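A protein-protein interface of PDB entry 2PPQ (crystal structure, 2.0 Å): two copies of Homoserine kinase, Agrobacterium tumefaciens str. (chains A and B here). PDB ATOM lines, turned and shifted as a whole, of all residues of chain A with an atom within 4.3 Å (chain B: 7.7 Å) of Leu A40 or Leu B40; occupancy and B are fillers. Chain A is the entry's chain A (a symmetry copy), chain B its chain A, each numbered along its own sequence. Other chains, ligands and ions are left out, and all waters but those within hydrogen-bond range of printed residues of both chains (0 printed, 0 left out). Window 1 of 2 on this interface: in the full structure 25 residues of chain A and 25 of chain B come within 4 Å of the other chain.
Printed residues of chain B that touch a printed residue of chain A: Ser B26, Gly B29, Ile B30, Leu B40, His B42 and Phe B104.
Hydrophobic or aromatic side chains of chain B within 4 Å of the printed part of chain A: Ile B30, Leu B40, His B42 and Phe B104.
Along chain B the printed residues that touch a printed residue of chain A span positions 26 to 104.
Among the printed residues, 8 pairs touch across the chains.
Among the printed residues, no Asp or Glu carboxylate lies within 4 Å of a Lys or Arg side-chain nitrogen of the other chain.
N of His A42 is in hydrogen-bond range of O of Ser A26 (2.9 Å).
N of His B42 lies within hydrogen-bond range of O of Ser B26 (2.9 Å).
The backbone carbonyl oxygen (O) of Lys A28 is in hydrogen-bond range of the backbone NH (N) of Leu A40 (2.9 Å).
O of Lys B28 lies within hydrogen-bond range of N of Leu B40 (2.9 Å).
O of Asn B38 is in hydrogen-bond range of N of Ile B30, at 3.0 Å.
A ring nitrogen (NE2) of His B42 lies within hydrogen-bond range of a ring nitrogen (NE2) of His A42 (2.9 Å).
Ile A30 touches its own counterpart, Ile B30.
Leu B40 touches its own counterpart, Leu A40.
His A42 touches its own counterpart, His B42.
His A42 touches Phe B104, and with the chains exchanged Phe A104 touches His B42.
Of the 8 pairs that touch across the chains among the printed residues, 7 have their exchanged pair printed and touching as well.
Leu A40 touches just one residue of chain B: Leu B40.
Of chain A, only Leu A40 (3.7 Å) comes within 4 Å of Leu B40.
Of the printed residues of chain B, Phe A104 touches Ser B26 (3.4 Å) and His B42 (3.6 Å).
Of the printed residues of chain B, Ile A30 touches Gly B29 (3.3 Å) and Ile B30 (3.8 Å).
The nearest residue of chain B that does not touch Leu A40 is His B42 (4.04 Å).
The nearest printed residue of chain A that does not touch Ile B30 is Lys A28 (4.1 Å).
Among the printed residues, pairs that only touch across the chains: Ile A30 with Gly B29, Phe A104 with Ser B26, Ser A26 with Phe B104, Phe A104 with His B42, His A42 with Phe B104, Leu A40 with Leu B40 and Ile A30 with Ile B30.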
ATOM      1  N   SER A  26      30.813 -25.401  -8.629  1.00  0.00           N
ATOM      2  CA  SER A  26      29.973 -24.378  -9.246  1.00  0.00           C
ATOM      3  C   SER A  26      28.732 -25.017  -9.877  1.00  0.00           C
ATOM      4  O   SER A  26      28.781 -26.165 -10.351  1.00  0.00           O
ATOM      5  CB  SER A  26      30.796 -23.611 -10.306  1.00  0.00           C
ATOM      6  OG  SER A  26      30.011 -22.796 -11.149  1.00  0.00           O
ATOM      7  N   TYR A  27      27.614 -24.290  -9.837  1.00  0.00           N
ATOM      8  CA  TYR A  27      26.460 -24.635 -10.652  1.00  0.00           C
ATOM      9  C   TYR A  27      25.636 -23.423 -11.074  1.00  0.00           C
ATOM     10  O   TYR A  27      25.417 -22.482 -10.304  1.00  0.00           O
ATOM     11  CB  TYR A  27      25.580 -25.717 -10.020  1.00  0.00           C
ATOM     12  CG  TYR A  27      24.780 -25.326  -8.813  1.00  0.00           C
ATOM     13  CD1 TYR A  27      23.422 -25.025  -8.914  1.00  0.00           C
ATOM     14  CD2 TYR A  27      25.367 -25.307  -7.557  1.00  0.00           C
ATOM     15  CE1 TYR A  27      22.673 -24.688  -7.785  1.00  0.00           C
ATOM     16  CE2 TYR A  27      24.630 -24.971  -6.412  1.00  0.00           C
ATOM     17  CZ  TYR A  27      23.293 -24.669  -6.535  1.00  0.00           C
ATOM     18  OH  TYR A  27      22.595 -24.347  -5.387  1.00  0.00           O
ATOM     19  N   LYS A  28      25.187 -23.489 -12.321  1.00  0.00           N
ATOM     20  CA  LYS A  28      24.561 -22.389 -13.016  1.00  0.00           C
ATOM     21  C   LYS A  28      23.359 -22.923 -13.766  1.00  0.00           C
ATOM     22  O   LYS A  28      23.494 -23.889 -14.513  1.00  0.00           O
ATOM     23  CB  LYS A  28      25.543 -21.830 -14.050  1.00  0.00           C
ATOM     24  CG  LYS A  28      26.214 -20.535 -13.696  1.00  0.00           C
ATOM     25  CD  LYS A  28      26.962 -20.558 -12.443  1.00  0.00           C
ATOM     26  CE  LYS A  28      28.104 -19.558 -12.503  1.00  0.00           C
ATOM     27  NZ  LYS A  28      28.590 -19.219 -11.154  1.00  0.00           N
ATOM     28  N   ILE A  30      21.141 -22.944 -16.894  1.00  0.00           N
ATOM     29  CA  ILE A  30      21.467 -22.595 -18.285  1.00  0.00           C
ATOM     30  C   ILE A  30      20.219 -22.557 -19.150  1.00  0.00           C
ATOM     31  O   ILE A  30      19.219 -23.200 -18.808  1.00  0.00           O
ATOM     32  CB  ILE A  30      22.546 -23.538 -18.900  1.00  0.00           C
ATOM     33  CG1 ILE A  30      22.103 -24.998 -18.866  1.00  0.00           C
ATOM     34  CG2 ILE A  30      23.895 -23.328 -18.174  1.00  0.00           C
ATOM     35  CD1 ILE A  30      23.110 -25.983 -19.485  1.00  0.00           C
ATOM     36  N   PHE A  39      21.189 -27.540 -15.573  1.00  0.00           N
ATOM     37  CA  PHE A  39      22.252 -26.878 -14.816  1.00  0.00           C
ATOM     38  C   PHE A  39      23.587 -27.376 -15.313  1.00  0.00           C
ATOM     39  O   PHE A  39      23.742 -28.558 -15.571  1.00  0.00           O
ATOM     40  CB  PHE A  39      22.121 -27.148 -13.315  1.00  0.00           C
ATOM     41  CG  PHE A  39      20.842 -26.635 -12.727  1.00  0.00           C
ATOM     42  CD1 PHE A  39      20.793 -25.391 -12.115  1.00  0.00           C
ATOM     43  CD2 PHE A  39      19.678 -27.385 -12.814  1.00  0.00           C
ATOM     44  CE1 PHE A  39      19.610 -24.914 -11.580  1.00  0.00           C
ATOM     45  CE2 PHE A  39      18.488 -26.907 -12.301  1.00  0.00           C
ATOM     46  CZ  PHE A  39      18.457 -25.666 -11.677  1.00  0.00           C
ATOM     47  N   LEU A  40      24.530 -26.449 -15.466  1.00  0.00           N
ATOM     48  CA  LEU A  40      25.910 -26.759 -15.790  1.00  0.00           C
ATOM     49  C   LEU A  40      26.671 -26.753 -14.486  1.00  0.00           C
ATOM     50  O   LEU A  40      26.731 -25.723 -13.799  1.00  0.00           O
ATOM     51  CB  LEU A  40      26.478 -25.724 -16.783  1.00  0.00           C
ATOM     52  CG  LEU A  40      27.968 -25.743 -17.167  1.00  0.00           C
ATOM     53  CD1 LEU A  40      28.485 -27.129 -17.430  1.00  0.00           C
ATOM     54  CD2 LEU A  40      28.157 -24.878 -18.416  1.00  0.00           C
ATOM     55  N   LEU A  41      27.208 -27.916 -14.135  1.00  0.00           N
ATOM     56  CA  LEU A  41      28.009 -28.107 -12.946  1.00  0.00           C
ATOM     57  C   LEU A  41      29.504 -28.116 -13.295  1.00  0.00           C
ATOM     58  O   LEU A  41      29.917 -28.684 -14.313  1.00  0.00           O
ATOM     59  CB  LEU A  41      27.643 -29.438 -12.261  1.00  0.00           C
ATOM     60  CG  LEU A  41      26.375 -29.494 -11.401  1.00  0.00           C
ATOM     61  CD1 LEU A  41      25.172 -28.979 -12.131  1.00  0.00           C
ATOM     62  CD2 LEU A  41      26.121 -30.929 -10.887  1.00  0.00           C
ATOM     63  N   HIS A  42      30.303 -27.469 -12.456  1.00  0.00           N
ATOM     64  CA  HIS A  42      31.736 -27.688 -12.438  1.00  0.00           C
ATOM     65  C   HIS A  42      32.068 -28.484 -11.185  1.00  0.00           C
ATOM     66  O   HIS A  42      31.436 -28.313 -10.139  1.00  0.00           O
ATOM     67  CB  HIS A  42      32.486 -26.364 -12.437  1.00  0.00           C
ATOM     68  CG  HIS A  42      32.355 -25.598 -13.722  1.00  0.00           C
ATOM     69  ND1 HIS A  42      32.973 -24.384 -13.930  1.00  0.00           N
ATOM     70  CD2 HIS A  42      31.682 -25.876 -14.860  1.00  0.00           C
ATOM     71  CE1 HIS A  42      32.689 -23.949 -15.144  1.00  0.00           C
ATOM     72  NE2 HIS A  42      31.907 -24.838 -15.730  1.00  0.00           N
ATOM     73  N   LEU A  48      29.586 -31.284 -15.727  1.00  0.00           N
ATOM     74  CA  LEU A  48      28.451 -32.184 -15.841  1.00  0.00           C
ATOM     75  C   LEU A  48      27.235 -31.381 -16.182  1.00  0.00           C
ATOM     76  O   LEU A  48      27.182 -30.158 -15.942  1.00  0.00           O
ATOM     77  CB  LEU A  48      28.190 -32.895 -14.497  1.00  0.00           C
ATOM     78  CG  LEU A  48      29.277 -33.801 -13.914  1.00  0.00           C
ATOM     79  CD1 LEU A  48      29.065 -34.042 -12.379  1.00  0.00           C
ATOM     80  CD2 LEU A  48      29.350 -35.117 -14.662  1.00  0.00           C
ATOM     81  N   ILE A  49      26.224 -32.074 -16.666  1.00  0.00           N
ATOM     82  CA  ILE A  49      24.921 -31.491 -16.846  1.00  0.00           C
ATOM     83  C   ILE A  49      23.956 -32.173 -15.865  1.00  0.00           C
ATOM     84  O   ILE A  49      23.943 -33.398 -15.731  1.00  0.00           O
ATOM     85  CB  ILE A  49      24.452 -31.625 -18.321  1.00  0.00           C
ATOM     86  CG1 ILE A  49      25.357 -30.798 -19.247  1.00  0.00           C
ATOM     87  CG2 ILE A  49      23.013 -31.201 -18.476  1.00  0.00           C
ATOM     88  CD1 ILE A  49      25.269 -29.296 -19.093  1.00  0.00           C
ATOM     89  N   PHE A 104      29.174 -34.125 -19.973  1.00  0.00           N
ATOM     90  CA  PHE A 104      29.198 -32.816 -20.637  1.00  0.00           C
ATOM     91  C   PHE A 104      29.869 -32.960 -21.997  1.00  0.00           C
ATOM     92  O   PHE A 104      30.971 -33.451 -22.064  1.00  0.00           O
ATOM     93  CB  PHE A 104      29.959 -31.812 -19.772  1.00  0.00           C
ATOM     94  CG  PHE A 104      30.004 -30.439 -20.348  1.00  0.00           C
ATOM     95  CD1 PHE A 104      28.973 -29.547 -20.119  1.00  0.00           C
ATOM     96  CD2 PHE A 104      31.073 -30.033 -21.115  1.00  0.00           C
ATOM     97  CE1 PHE A 104      28.999 -28.274 -20.655  1.00  0.00           C
ATOM     98  CE2 PHE A 104      31.095 -28.753 -21.670  1.00  0.00           C
ATOM     99  CZ  PHE A 104      30.059 -27.874 -21.429  1.00  0.00           C
ATOM    100  N   LEU B  12      31.650 -14.514 -31.653  1.00  0.00           N
ATOM    101  CA  LEU B  12      32.286 -14.774 -30.360  1.00  0.00           C
ATOM    102  C   LEU B  12      33.765 -15.163 -30.562  1.00  0.00           C
ATOM    103  O   LEU B  12      34.640 -14.675 -29.851  1.00  0.00           O
ATOM    104  CB  LEU B  12      31.507 -15.845 -29.585  1.00  0.00           C
ATOM    105  CG  LEU B  12      31.972 -16.216 -28.175  1.00  0.00           C
ATOM    106  CD1 LEU B  12      32.311 -15.011 -27.323  1.00  0.00           C
ATOM    107  CD2 LEU B  12      30.921 -17.081 -27.463  1.00  0.00           C
ATOM    108  N   LEU B  24      37.810 -21.113 -27.754  1.00  0.00           N
ATOM    109  CA  LEU B  24      36.445 -21.454 -27.359  1.00  0.00           C
ATOM    110  C   LEU B  24      36.102 -22.936 -27.563  1.00  0.00           C
ATOM    111  O   LEU B  24      36.259 -23.471 -28.673  1.00  0.00           O
ATOM    112  CB  LEU B  24      35.451 -20.591 -28.140  1.00  0.00           C
ATOM    113  CG  LEU B  24      34.008 -20.634 -27.653  1.00  0.00           C
ATOM    114  CD1 LEU B  24      33.949 -20.136 -26.208  1.00  0.00           C
ATOM    115  CD2 LEU B  24      33.084 -19.827 -28.571  1.00  0.00           C
ATOM    116  N   SER B  26      33.045 -24.154 -25.702  1.00  0.00           N
ATOM    117  CA  SER B  26      31.639 -24.193 -25.306  1.00  0.00           C
ATOM    118  C   SER B  26      31.176 -22.808 -24.844  1.00  0.00           C
ATOM    119  O   SER B  26      31.968 -22.028 -24.286  1.00  0.00           O
ATOM    120  CB  SER B  26      31.453 -25.239 -24.184  1.00  0.00           C
ATOM    121  OG  SER B  26      30.198 -25.161 -23.542  1.00  0.00           O
ATOM    122  N   TYR B  27      29.911 -22.491 -25.119  1.00  0.00           N
ATOM    123  CA  TYR B  27      29.261 -21.356 -24.482  1.00  0.00           C
ATOM    124  C   TYR B  27      27.761 -21.549 -24.289  1.00  0.00           C
ATOM    125  O   TYR B  27      27.056 -22.086 -25.151  1.00  0.00           O
ATOM    126  CB  TYR B  27      29.570 -20.023 -25.170  1.00  0.00           C
ATOM    127  CG  TYR B  27      28.951 -19.792 -26.518  1.00  0.00           C
ATOM    128  CD1 TYR B  27      27.812 -19.000 -26.663  1.00  0.00           C
ATOM    129  CD2 TYR B  27      29.533 -20.323 -27.658  1.00  0.00           C
ATOM    130  CE1 TYR B  27      27.255 -18.765 -27.920  1.00  0.00           C
ATOM    131  CE2 TYR B  27      28.987 -20.098 -28.930  1.00  0.00           C
ATOM    132  CZ  TYR B  27      27.858 -19.319 -29.050  1.00  0.00           C
ATOM    133  OH  TYR B  27      27.348 -19.112 -30.317  1.00  0.00           O
ATOM    134  N   LYS B  28      27.306 -21.087 -23.132  1.00  0.00           N
ATOM    135  CA  LYS B  28      25.974 -21.330 -22.630  1.00  0.00           C
ATOM    136  C   LYS B  28      25.441 -20.036 -22.051  1.00  0.00           C
ATOM    137  O   LYS B  28      26.113 -19.423 -21.224  1.00  0.00           O
ATOM    138  CB  LYS B  28      26.049 -22.352 -21.491  1.00  0.00           C
ATOM    139  CG  LYS B  28      25.608 -23.747 -21.823  1.00  0.00           C
ATOM    140  CD  LYS B  28      26.328 -24.368 -22.931  1.00  0.00           C
ATOM    141  CE  LYS B  28      26.348 -25.877 -22.756  1.00  0.00           C
ATOM    142  NZ  LYS B  28      26.645 -26.558 -24.028  1.00  0.00           N
ATOM    143  N   GLY B  29      24.243 -19.630 -22.457  1.00  0.00           N
ATOM    144  CA  GLY B  29      23.523 -18.561 -21.747  1.00  0.00           C
ATOM    145  C   GLY B  29      23.228 -19.029 -20.325  1.00  0.00           C
ATOM    146  O   GLY B  29      22.808 -20.165 -20.124  1.00  0.00           O
ATOM    147  N   ILE B  30      23.469 -18.179 -19.336  1.00  0.00           N
ATOM    148  CA  ILE B  30      23.203 -18.555 -17.939  1.00  0.00           C
ATOM    149  C   ILE B  30      22.203 -17.608 -17.297  1.00  0.00           C
ATOM    150  O   ILE B  30      22.064 -16.467 -17.750  1.00  0.00           O
ATOM    151  CB  ILE B  30      24.506 -18.656 -17.089  1.00  0.00           C
ATOM    152  CG1 ILE B  30      25.282 -17.341 -17.091  1.00  0.00           C
ATOM    153  CG2 ILE B  30      25.369 -19.834 -17.597  1.00  0.00           C
ATOM    154  CD1 ILE B  30      26.568 -17.360 -16.245  1.00  0.00           C
ATOM    155  N   ASN B  38      24.453 -12.825 -19.774  1.00  0.00           N
ATOM    156  CA  ASN B  38      25.664 -13.483 -19.326  1.00  0.00           C
ATOM    157  C   ASN B  38      25.826 -14.867 -19.946  1.00  0.00           C
ATOM    158  O   ASN B  38      24.848 -15.612 -20.119  1.00  0.00           O
ATOM    159  CB  ASN B  38      25.705 -13.544 -17.802  1.00  0.00           C
ATOM    160  CG  ASN B  38      25.754 -12.163 -17.162  1.00  0.00           C
ATOM    161  OD1 ASN B  38      26.707 -11.417 -17.357  1.00  0.00           O
ATOM    162  ND2 ASN B  38      24.714 -11.812 -16.404  1.00  0.00           N
ATOM    163  N   PHE B  39      27.069 -15.182 -20.297  1.00  0.00           N
ATOM    164  CA  PHE B  39      27.417 -16.461 -20.915  1.00  0.00           C
ATOM    165  C   PHE B  39      28.585 -17.060 -20.171  1.00  0.00           C
ATOM    166  O   PHE B  39      29.507 -16.350 -19.807  1.00  0.00           O
ATOM    167  CB  PHE B  39      27.774 -16.290 -22.394  1.00  0.00           C
ATOM    168  CG  PHE B  39      26.645 -15.749 -23.219  1.00  0.00           C
ATOM    169  CD1 PHE B  39      25.807 -16.604 -23.919  1.00  0.00           C
ATOM    170  CD2 PHE B  39      26.405 -14.383 -23.271  1.00  0.00           C
ATOM    171  CE1 PHE B  39      24.761 -16.104 -24.674  1.00  0.00           C
ATOM    172  CE2 PHE B  39      25.350 -13.878 -24.005  1.00  0.00           C
ATOM    173  CZ  PHE B  39      24.527 -14.745 -24.714  1.00  0.00           C
ATOM    174  N   LEU B  40      28.511 -18.367 -19.932  1.00  0.00           N
ATOM    175  CA  LEU B  40      29.601 -19.139 -19.365  1.00  0.00           C
ATOM    176  C   LEU B  40      30.316 -19.793 -20.523  1.00  0.00           C
ATOM    177  O   LEU B  40      29.718 -20.586 -21.263  1.00  0.00           O
ATOM    178  CB  LEU B  40      29.060 -20.186 -18.369  1.00  0.00           C
ATOM    179  CG  LEU B  40      30.001 -21.232 -17.745  1.00  0.00           C
ATOM    180  CD1 LEU B  40      31.312 -20.647 -17.302  1.00  0.00           C
ATOM    181  CD2 LEU B  40      29.291 -21.869 -16.547  1.00  0.00           C
ATOM    182  N   LEU B  41      31.578 -19.417 -20.697  1.00  0.00           N
ATOM    183  CA  LEU B  41      32.445 -19.957 -21.721  1.00  0.00           C
ATOM    184  C   LEU B  41      33.388 -21.015 -21.132  1.00  0.00           C
ATOM    185  O   LEU B  41      33.909 -20.856 -20.021  1.00  0.00           O
ATOM    186  CB  LEU B  41      33.285 -18.833 -22.359  1.00  0.00           C
ATOM    187  CG  LEU B  41      32.624 -17.932 -23.409  1.00  0.00           C
ATOM    188  CD1 LEU B  41      31.330 -17.353 -22.926  1.00  0.00           C
ATOM    189  CD2 LEU B  41      33.586 -16.808 -23.853  1.00  0.00           C
ATOM    190  N   HIS B  42      33.585 -22.098 -21.872  1.00  0.00           N
ATOM    191  CA  HIS B  42      34.700 -22.996 -21.639  1.00  0.00           C
ATOM    192  C   HIS B  42      35.706 -22.786 -22.760  1.00  0.00           C
ATOM    193  O   HIS B  42      35.333 -22.517 -23.904  1.00  0.00           O
ATOM    194  CB  HIS B  42      34.233 -24.444 -21.611  1.00  0.00           C
ATOM    195  CG  HIS B  42      33.376 -24.777 -20.424  1.00  0.00           C
ATOM    196  ND1 HIS B  42      32.867 -26.039 -20.205  1.00  0.00           N
ATOM    197  CD2 HIS B  42      32.944 -24.016 -19.395  1.00  0.00           C
ATOM    198  CE1 HIS B  42      32.162 -26.040 -19.089  1.00  0.00           C
ATOM    199  NE2 HIS B  42      32.194 -24.824 -18.577  1.00  0.00           N
ATOM    200  N   THR B  43      36.981 -22.897 -22.411  1.00  0.00           N
ATOM    201  CA  THR B  43      38.070 -22.709 -23.348  1.00  0.00           C
ATOM    202  C   THR B  43      39.096 -23.823 -23.132  1.00  0.00           C
ATOM    203  O   THR B  43      38.941 -24.660 -22.249  1.00  0.00           O
ATOM    204  CB  THR B  43      38.776 -21.317 -23.192  1.00  0.00           C
ATOM    205  OG1 THR B  43      39.546 -21.284 -21.986  1.00  0.00           O
ATOM    206  CG2 THR B  43      37.784 -20.158 -23.207  1.00  0.00           C
ATOM    207  N   ASP B  46      41.189 -21.483 -19.232  1.00  0.00           N
ATOM    208  CA  ASP B  46      40.211 -21.369 -18.118  1.00  0.00           C
ATOM    209  C   ASP B  46      38.810 -21.029 -18.598  1.00  0.00           C
ATOM    210  O   ASP B  46      38.642 -20.435 -19.662  1.00  0.00           O
ATOM    211  CB  ASP B  46      40.632 -20.268 -17.149  1.00  0.00           C
ATOM    212  CG  ASP B  46      41.971 -20.542 -16.512  1.00  0.00           C
ATOM    213  OD1 ASP B  46      42.061 -21.495 -15.699  1.00  0.00           O
ATOM    214  OD2 ASP B  46      42.921 -19.798 -16.824  1.00  0.00           O
ATOM    215  N   PRO B  47      37.792 -21.346 -17.776  1.00  0.00           N
ATOM    216  CA  PRO B  47      36.464 -20.865 -18.110  1.00  0.00           C
ATOM    217  C   PRO B  47      36.364 -19.345 -17.897  1.00  0.00           C
ATOM    218  O   PRO B  47      37.202 -18.733 -17.215  1.00  0.00           O
ATOM    219  CB  PRO B  47      35.548 -21.640 -17.155  1.00  0.00           C
ATOM    220  CG  PRO B  47      36.407 -21.939 -15.974  1.00  0.00           C
ATOM    221  CD  PRO B  47      37.806 -22.121 -16.524  1.00  0.00           C
ATOM    222  N   LEU B  48      35.352 -18.744 -18.498  1.00  0.00           N
ATOM    223  CA  LEU B  48      35.236 -17.296 -18.507  1.00  0.00           C
ATOM    224  C   LEU B  48      33.786 -16.931 -18.429  1.00  0.00           C
ATOM    225  O   LEU B  48      32.899 -17.742 -18.762  1.00  0.00           O
ATOM    226  CB  LEU B  48      35.801 -16.718 -19.821  1.00  0.00           C
ATOM    227  CG  LEU B  48      37.280 -16.936 -20.150  1.00  0.00           C
ATOM    228  CD1 LEU B  48      37.567 -16.728 -21.678  1.00  0.00           C
ATOM    229  CD2 LEU B  48      38.165 -16.040 -19.308  1.00  0.00           C
ATOM    230  N   ILE B  49      33.540 -15.687 -18.069  1.00  0.00           N
ATOM    231  CA  ILE B  49      32.219 -15.122 -18.148  1.00  0.00           C
ATOM    232  C   ILE B  49      32.237 -14.024 -19.222  1.00  0.00           C
ATOM    233  O   ILE B  49      33.144 -13.191 -19.268  1.00  0.00           O
ATOM    234  CB  ILE B  49      31.764 -14.582 -16.764  1.00  0.00           C
ATOM    235  CG1 ILE B  49      31.610 -15.738 -15.764  1.00  0.00           C
ATOM    236  CG2 ILE B  49      30.473 -13.810 -16.879  1.00  0.00           C
ATOM    237  CD1 ILE B  49      30.482 -16.708 -16.038  1.00  0.00           C
ATOM    238  N   LEU B  50      31.255 -14.070 -20.116  1.00  0.00           N
ATOM    239  CA  LEU B  50      31.012 -12.989 -21.072  1.00  0.00           C
ATOM    240  C   LEU B  50      29.755 -12.257 -20.651  1.00  0.00           C
ATOM    241  O   LEU B  50      28.688 -12.883 -20.482  1.00  0.00           O
ATOM    242  CB  LEU B  50      30.829 -13.546 -22.500  1.00  0.00           C
ATOM    243  CG  LEU B  50      30.346 -12.612 -23.626  1.00  0.00           C
ATOM    244  CD1 LEU B  50      31.358 -11.497 -23.934  1.00  0.00           C
ATOM    245  CD2 LEU B  50      30.092 -13.438 -24.905  1.00  0.00           C
ATOM    246  N   THR B  51      29.867 -10.936 -20.536  1.00  0.00           N
ATOM    247  CA  THR B  51      28.757 -10.086 -20.160  1.00  0.00           C
ATOM    248  C   THR B  51      28.443  -9.088 -21.269  1.00  0.00           C
ATOM    249  O   THR B  51      29.314  -8.346 -21.711  1.00  0.00           O
ATOM    250  CB  THR B  51      29.070  -9.349 -18.838  1.00  0.00           C
ATOM    251  OG1 THR B  51      29.414 -10.317 -17.838  1.00  0.00           O
ATOM    252  CG2 THR B  51      27.883  -8.538 -18.381  1.00  0.00           C
ATOM    253  N   PHE B 104      36.452 -16.205 -14.183  1.00  0.00           N
ATOM    254  CA  PHE B 104      35.405 -17.065 -13.620  1.00  0.00           C
ATOM    255  C   PHE B 104      35.733 -17.358 -12.162  1.00  0.00           C
ATOM    256  O   PHE B 104      36.812 -17.823 -11.880  1.00  0.00           O
ATOM    257  CB  PHE B 104      35.321 -18.365 -14.419  1.00  0.00           C
ATOM    258  CG  PHE B 104      34.255 -19.291 -13.944  1.00  0.00           C
ATOM    259  CD1 PHE B 104      32.957 -19.163 -14.402  1.00  0.00           C
ATOM    260  CD2 PHE B 104      34.544 -20.292 -13.043  1.00  0.00           C
ATOM    261  CE1 PHE B 104      31.958 -20.010 -13.962  1.00  0.00           C
ATOM    262  CE2 PHE B 104      33.533 -21.139 -12.585  1.00  0.00           C
ATOM    263  CZ  PHE B 104      32.244 -21.000 -13.055  1.00  0.00           C
